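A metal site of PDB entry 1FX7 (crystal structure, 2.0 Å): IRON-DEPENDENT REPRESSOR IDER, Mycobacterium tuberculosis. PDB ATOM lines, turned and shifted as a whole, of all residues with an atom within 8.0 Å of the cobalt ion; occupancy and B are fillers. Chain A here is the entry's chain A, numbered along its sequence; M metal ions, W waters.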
ATOM      1  N   GLU A   3       8.417  -8.627  14.486  1.00  0.00           N
ATOM      2  CA  GLU A   3       9.530  -8.089  15.281  1.00  0.00           C
ATOM      3  C   GLU A   3       9.071  -7.167  16.419  1.00  0.00           C
ATOM      4  O   GLU A   3       9.741  -7.058  17.443  1.00  0.00           O
ATOM      5  CB  GLU A   3      10.538  -7.402  14.361  1.00  0.00           C
ATOM      6  CG  GLU A   3      11.934  -7.315  14.959  1.00  0.00           C
ATOM      7  CD  GLU A   3      13.059  -7.326  13.945  1.00  0.00           C
ATOM      8  OE1 GLU A   3      13.002  -6.549  12.958  1.00  0.00           O
ATOM      9  OE2 GLU A   3      14.019  -8.105  14.129  1.00  0.00           O
ATOM     10  N   LEU A   4       7.915  -6.536  16.299  1.00  0.00           N
ATOM     11  CA  LEU A   4       7.329  -5.706  17.309  1.00  0.00           C
ATOM     12  C   LEU A   4       6.628  -6.526  18.380  1.00  0.00           C
ATOM     13  O   LEU A   4       6.230  -5.994  19.426  1.00  0.00           O
ATOM     14  CB  LEU A   4       6.291  -4.760  16.675  1.00  0.00           C
ATOM     15  CG  LEU A   4       6.861  -3.787  15.627  1.00  0.00           C
ATOM     16  CD1 LEU A   4       5.744  -2.950  15.047  1.00  0.00           C
ATOM     17  CD2 LEU A   4       7.923  -2.876  16.253  1.00  0.00           C
ATOM     18  N   VAL A   5       6.385  -7.814  18.151  1.00  0.00           N
ATOM     19  CA  VAL A   5       5.697  -8.750  19.025  1.00  0.00           C
ATOM     20  C   VAL A   5       4.203  -8.468  19.067  1.00  0.00           C
ATOM     21  O   VAL A   5       3.386  -9.361  18.808  1.00  0.00           O
ATOM     22  CB  VAL A   5       6.234  -8.835  20.464  1.00  0.00           C
ATOM     23  CG1 VAL A   5       5.593 -10.005  21.203  1.00  0.00           C
ATOM     24  CG2 VAL A   5       7.753  -9.042  20.517  1.00  0.00           C
ATOM     25  N   ASP A   6       3.802  -7.258  19.452  1.00  0.00           N
ATOM     26  CA  ASP A   6       2.411  -6.847  19.512  1.00  0.00           C
ATOM     27  C   ASP A   6       2.366  -5.443  18.913  1.00  0.00           C
ATOM     28  O   ASP A   6       2.769  -4.472  19.563  1.00  0.00           O
ATOM     29  CB  ASP A   6       1.857  -6.873  20.926  1.00  0.00           C
ATOM     30  CG  ASP A   6       0.391  -6.563  21.029  1.00  0.00           C
ATOM     31  OD1 ASP A   6      -0.269  -7.194  21.897  1.00  0.00           O
ATOM     32  OD2 ASP A   6      -0.150  -5.688  20.320  1.00  0.00           O
ATOM     33  N   THR A   7       1.930  -5.368  17.662  1.00  0.00           N
ATOM     34  CA  THR A   7       1.911  -4.095  16.961  1.00  0.00           C
ATOM     35  C   THR A   7       1.032  -3.051  17.619  1.00  0.00           C
ATOM     36  O   THR A   7       1.502  -1.917  17.757  1.00  0.00           O
ATOM     37  CB  THR A   7       1.518  -4.252  15.472  1.00  0.00           C
ATOM     38  OG1 THR A   7       2.449  -5.169  14.887  1.00  0.00           O
ATOM     39  CG2 THR A   7       1.579  -2.919  14.765  1.00  0.00           C
ATOM     40  N   GLU A   9       0.170  -2.733  20.675  1.00  0.00           N
ATOM     41  CA  GLU A   9       0.802  -2.288  21.935  1.00  0.00           C
ATOM     42  C   GLU A   9       1.984  -1.390  21.663  1.00  0.00           C
ATOM     43  O   GLU A   9       2.116  -0.399  22.395  1.00  0.00           O
ATOM     44  CB  GLU A   9       1.177  -3.486  22.817  1.00  0.00           C
ATOM     45  CG  GLU A   9      -0.072  -4.123  23.452  1.00  0.00           C
ATOM     46  CD  GLU A   9       0.303  -5.194  24.460  1.00  0.00           C
ATOM     47  OE1 GLU A   9       1.482  -5.601  24.483  1.00  0.00           O
ATOM     48  OE2 GLU A   9      -0.601  -5.645  25.200  1.00  0.00           O
ATOM     49  N   MET A  10       2.749  -1.579  20.582  1.00  0.00           N
ATOM     50  CA  MET A  10       3.870  -0.676  20.301  1.00  0.00           C
ATOM     51  C   MET A  10       3.458   0.721  19.876  1.00  0.00           C
ATOM     52  O   MET A  10       3.985   1.782  20.185  1.00  0.00           O
ATOM     53  CB  MET A  10       4.835  -1.328  19.309  1.00  0.00           C
ATOM     54  CG  MET A  10       5.739  -2.345  20.005  1.00  0.00           C
ATOM     55  SD  MET A  10       6.483  -1.699  21.529  1.00  0.00           S
ATOM     56  CE  MET A  10       7.710  -0.582  20.837  1.00  0.00           C
ATOM     57  N   TYR A  11       2.278   0.776  19.208  1.00  0.00           N
ATOM     58  CA  TYR A  11       1.604   1.993  18.760  1.00  0.00           C
ATOM     59  C   TYR A  11       1.177   2.810  19.978  1.00  0.00           C
ATOM     60  O   TYR A  11       1.461   4.012  20.082  1.00  0.00           O
ATOM     61  CB  TYR A  11       0.412   1.655  17.867  1.00  0.00           C
ATOM     62  CG  TYR A  11       0.735   1.563  16.397  1.00  0.00           C
ATOM     63  CD1 TYR A  11       1.533   0.573  15.864  1.00  0.00           C
ATOM     64  CD2 TYR A  11       0.163   2.481  15.515  1.00  0.00           C
ATOM     65  CE1 TYR A  11       1.824   0.510  14.507  1.00  0.00           C
ATOM     66  CE2 TYR A  11       0.437   2.434  14.154  1.00  0.00           C
ATOM     67  CZ  TYR A  11       1.248   1.444  13.663  1.00  0.00           C
ATOM     68  OH  TYR A  11       1.502   1.403  12.309  1.00  0.00           O
ATOM     69  N   ARG A  13       2.289   2.398  23.179  1.00  0.00           N
ATOM     70  CA  ARG A  13       3.446   2.867  23.927  1.00  0.00           C
ATOM     71  C   ARG A  13       4.263   3.904  23.180  1.00  0.00           C
ATOM     72  O   ARG A  13       4.884   4.706  23.892  1.00  0.00           O
ATOM     73  CB  ARG A  13       4.353   1.725  24.417  1.00  0.00           C
ATOM     74  CG  ARG A  13       5.052   2.134  25.722  1.00  0.00           C
ATOM     75  CD  ARG A  13       6.362   1.402  25.887  1.00  0.00           C
ATOM     76  NE  ARG A  13       7.415   2.026  25.094  1.00  0.00           N
ATOM     77  CZ  ARG A  13       8.413   1.402  24.499  1.00  0.00           C
ATOM     78  NH1 ARG A  13       8.548   0.081  24.581  1.00  0.00           N
ATOM     79  NH2 ARG A  13       9.319   2.074  23.782  1.00  0.00           N
ATOM     80  N   THR A  14       4.311   3.920  21.830  1.00  0.00           N
ATOM     81  CA  THR A  14       5.049   4.974  21.141  1.00  0.00           C
ATOM     82  C   THR A  14       4.398   6.321  21.362  1.00  0.00           C
ATOM     83  O   THR A  14       5.087   7.321  21.609  1.00  0.00           O
ATOM     84  CB  THR A  14       5.208   4.662  19.626  1.00  0.00           C
ATOM     85  OG1 THR A  14       5.897   3.421  19.529  1.00  0.00           O
ATOM     86  CG2 THR A  14       6.018   5.711  18.876  1.00  0.00           C
ATOM     87  N   LEU A  34       8.759   2.788  14.356  1.00  0.00           N
ATOM     88  CA  LEU A  34       8.382   1.381  14.236  1.00  0.00           C
ATOM     89  C   LEU A  34       8.740   0.810  12.874  1.00  0.00           C
ATOM     90  O   LEU A  34       8.477  -0.353  12.585  1.00  0.00           O
ATOM     91  CB  LEU A  34       6.907   1.187  14.598  1.00  0.00           C
ATOM     92  CG  LEU A  34       6.533   1.654  16.022  1.00  0.00           C
ATOM     93  CD1 LEU A  34       5.083   1.336  16.354  1.00  0.00           C
ATOM     94  CD2 LEU A  34       7.502   1.066  17.048  1.00  0.00           C
ATOM     95  N   VAL A  75       1.313  -1.561  29.382  1.00  0.00           N
ATOM     96  CA  VAL A  75       2.500  -1.971  28.622  1.00  0.00           C
ATOM     97  C   VAL A  75       3.754  -1.344  29.220  1.00  0.00           C
ATOM     98  O   VAL A  75       4.769  -2.028  29.471  1.00  0.00           O
ATOM     99  CB  VAL A  75       2.391  -1.560  27.137  1.00  0.00           C
ATOM    100  CG1 VAL A  75       3.662  -1.913  26.341  1.00  0.00           C
ATOM    101  CG2 VAL A  75       1.180  -2.214  26.487  1.00  0.00           C
ATOM    102  N   HIS A  79       6.973  -2.986  30.858  1.00  0.00           N
ATOM    103  CA  HIS A  79       8.308  -2.718  30.324  1.00  0.00           C
ATOM    104  C   HIS A  79       9.298  -2.407  31.437  1.00  0.00           C
ATOM    105  O   HIS A  79      10.402  -2.946  31.508  1.00  0.00           O
ATOM    106  CB  HIS A  79       8.208  -1.483  29.424  1.00  0.00           C
ATOM    107  CG  HIS A  79       9.529  -1.125  28.805  1.00  0.00           C
ATOM    108  ND1 HIS A  79       9.980  -1.723  27.653  1.00  0.00           N
ATOM    109  CD2 HIS A  79      10.485  -0.231  29.165  1.00  0.00           C
ATOM    110  CE1 HIS A  79      11.157  -1.235  27.333  1.00  0.00           C
ATOM    111  NE2 HIS A  79      11.480  -0.323  28.234  1.00  0.00           N
ATOM    112  N   HIS A  98      16.857  -2.551  27.650  1.00  0.00           N
ATOM    113  CA  HIS A  98      15.726  -1.930  26.944  1.00  0.00           C
ATOM    114  C   HIS A  98      15.246  -2.772  25.778  1.00  0.00           C
ATOM    115  O   HIS A  98      14.009  -2.972  25.665  1.00  0.00           O
ATOM    116  CB  HIS A  98      16.069  -0.492  26.516  1.00  0.00           C
ATOM    117  CG  HIS A  98      14.953   0.048  25.660  1.00  0.00           C
ATOM    118  ND1 HIS A  98      13.766   0.468  26.194  1.00  0.00           N
ATOM    119  CD2 HIS A  98      14.865   0.184  24.306  1.00  0.00           C
ATOM    120  CE1 HIS A  98      12.981   0.862  25.200  1.00  0.00           C
ATOM    121  NE2 HIS A  98      13.629   0.699  24.048  1.00  0.00           N
ATOM    122  N   ALA A  99      16.124  -3.245  24.893  1.00  0.00           N
ATOM    123  CA  ALA A  99      15.618  -4.015  23.744  1.00  0.00           C
ATOM    124  C   ALA A  99      14.942  -5.306  24.199  1.00  0.00           C
ATOM    125  O   ALA A  99      13.922  -5.734  23.636  1.00  0.00           O
ATOM    126  CB  ALA A  99      16.722  -4.270  22.728  1.00  0.00           C
ATOM    127  N   GLU A 100      15.500  -5.959  25.207  1.00  0.00           N
ATOM    128  CA  GLU A 100      14.900  -7.179  25.754  1.00  0.00           C
ATOM    129  C   GLU A 100      13.519  -6.880  26.318  1.00  0.00           C
ATOM    130  O   GLU A 100      12.504  -7.496  25.985  1.00  0.00           O
ATOM    131  CB  GLU A 100      15.816  -7.725  26.848  1.00  0.00           C
ATOM    132  CG  GLU A 100      15.411  -9.108  27.352  1.00  0.00           C
ATOM    133  CD  GLU A 100      15.996 -10.234  26.513  1.00  0.00           C
ATOM    134  OE1 GLU A 100      17.140 -10.095  26.041  1.00  0.00           O
ATOM    135  OE2 GLU A 100      15.337 -11.278  26.326  1.00  0.00           O
ATOM    136  N   ALA A 101      13.441  -5.851  27.169  1.00  0.00           N
ATOM    137  CA  ALA A 101      12.160  -5.461  27.776  1.00  0.00           C
ATOM    138  C   ALA A 101      11.140  -4.995  26.739  1.00  0.00           C
ATOM    139  O   ALA A 101       9.936  -5.173  26.954  1.00  0.00           O
ATOM    140  CB  ALA A 101      12.363  -4.356  28.818  1.00  0.00           C
ATOM    141  N   CYS A 102      11.563  -4.449  25.595  1.00  0.00           N
ATOM    142  CA  CYS A 102      10.622  -4.036  24.566  1.00  0.00           C
ATOM    143  C   CYS A 102       9.882  -5.251  23.984  1.00  0.00           C
ATOM    144  O   CYS A 102       8.773  -5.109  23.456  1.00  0.00           O
ATOM    145  CB  CYS A 102      11.228  -3.240  23.404  1.00  0.00           C
ATOM    146  SG  CYS A 102       9.964  -2.402  22.396  1.00  0.00           S
ATOM    147  N   ARG A 103      10.481  -6.423  24.028  1.00  0.00           N
ATOM    148  CA  ARG A 103       9.840  -7.676  23.667  1.00  0.00           C
ATOM    149  C   ARG A 103       9.066  -8.232  24.887  1.00  0.00           C
ATOM    150  O   ARG A 103       7.902  -8.611  24.746  1.00  0.00           O
ATOM    151  CB  ARG A 103      10.886  -8.693  23.233  1.00  0.00           C
ATOM    152  CG  ARG A 103      11.698  -8.285  21.988  1.00  0.00           C
ATOM    153  CD  ARG A 103      12.348  -9.515  21.344  1.00  0.00           C
ATOM    154  NE  ARG A 103      13.308 -10.132  22.261  1.00  0.00           N
ATOM    155  CZ  ARG A 103      14.510  -9.677  22.539  1.00  0.00           C
ATOM    156  NH1 ARG A 103      15.251 -10.351  23.422  1.00  0.00           N
ATOM    157  NH2 ARG A 103      14.994  -8.588  21.922  1.00  0.00           N
ATOM    158  N   TRP A 104       9.667  -8.234  26.080  1.00  0.00           N
ATOM    159  CA  TRP A 104       8.987  -8.833  27.236  1.00  0.00           C
ATOM    160  C   TRP A 104       7.726  -8.120  27.671  1.00  0.00           C
ATOM    161  O   TRP A 104       6.758  -8.757  28.131  1.00  0.00           O
ATOM    162  CB  TRP A 104       9.898  -8.906  28.470  1.00  0.00           C
ATOM    163  CG  TRP A 104      11.019  -9.885  28.327  1.00  0.00           C
ATOM    164  CD1 TRP A 104      11.625 -10.286  27.180  1.00  0.00           C
ATOM    165  CD2 TRP A 104      11.731 -10.555  29.389  1.00  0.00           C
ATOM    166  NE1 TRP A 104      12.641 -11.157  27.446  1.00  0.00           N
ATOM    167  CE2 TRP A 104      12.728 -11.346  28.786  1.00  0.00           C
ATOM    168  CE3 TRP A 104      11.604 -10.566  30.778  1.00  0.00           C
ATOM    169  CZ2 TRP A 104      13.609 -12.145  29.522  1.00  0.00           C
ATOM    170  CZ3 TRP A 104      12.475 -11.363  31.512  1.00  0.00           C
ATOM    171  CH2 TRP A 104      13.463 -12.133  30.875  1.00  0.00           C
ATOM    172  N   GLU A 105       7.648  -6.809  27.425  1.00  0.00           N
ATOM    173  CA  GLU A 105       6.477  -6.040  27.845  1.00  0.00           C
ATOM    174  C   GLU A 105       5.195  -6.546  27.226  1.00  0.00           C
ATOM    175  O   GLU A 105       4.127  -6.214  27.727  1.00  0.00           O
ATOM    176  CB  GLU A 105       6.702  -4.544  27.464  1.00  0.00           C
ATOM    177  CG  GLU A 105       6.625  -4.311  25.946  1.00  0.00           C
ATOM    178  CD  GLU A 105       7.163  -2.945  25.554  1.00  0.00           C
ATOM    179  OE1 GLU A 105       7.451  -2.138  26.444  1.00  0.00           O
ATOM    180  OE2 GLU A 105       7.345  -2.640  24.348  1.00  0.00           O
ATOM    181  N   HIS A 106       5.273  -7.249  26.077  1.00  0.00           N
ATOM    182  CA  HIS A 106       4.066  -7.697  25.411  1.00  0.00           C
ATOM    183  C   HIS A 106       3.591  -9.089  25.825  1.00  0.00           C
ATOM    184  O   HIS A 106       2.548  -9.537  25.303  1.00  0.00           O
ATOM    185  CB  HIS A 106       4.308  -7.700  23.877  1.00  0.00           C
ATOM    186  CG  HIS A 106       4.829  -6.354  23.434  1.00  0.00           C
ATOM    187  ND1 HIS A 106       4.087  -5.216  23.497  1.00  0.00           N
ATOM    188  CD2 HIS A 106       6.039  -6.017  22.935  1.00  0.00           C
ATOM    189  CE1 HIS A 106       4.809  -4.186  23.053  1.00  0.00           C
ATOM    190  NE2 HIS A 106       5.997  -4.653  22.688  1.00  0.00           N
HETATM  191 CO    CO M   1       7.794  -3.469  22.616  1.00  0.00          CO
HETATM  192  O   HOH W   1       8.201  -4.432  20.559  1.00  0.00           O
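The side-chain hydroxyl (OG1) of Thr 14 is in hydrogen-bond range of the backbone carbonyl oxygen (O) of Met 10. OE1 of Glu 9 lies within hydrogen-bond range of ND1 of His 106 (2.8 Å). OE1 of Glu 105 is in hydrogen-bond range of ND1 of His 79, 2.8 Å away. NH1 of Arg 13 is in salt-bridge range of OE1 of Glu 105. The side-chain sulfur (SG) of Cys 102 lies close to the guanidinium group (NH1) of Arg 13 (3.6 Å).
The cobalt ion is bound by the side-chain carboxylate of Glu 105 (2.0 Å), the backbone carbonyl oxygen of Cys 102 (2.1 Å), a ring nitrogen (NE2) of His 106 (2.2 Å), water W1 (2.3 Å), the side-chain sulfur of Cys 102 (2.4 Å) and the side-chain sulfur of Met 10 (2.5 Å). The cobalt ion has six donor atoms within binding distance.
Within 4 Å of the cobalt ion: Met 10, Cys 102, Glu 105 and His 106. Along chain A the residues within 4 Å of the cobalt ion span positions 10 to 106.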
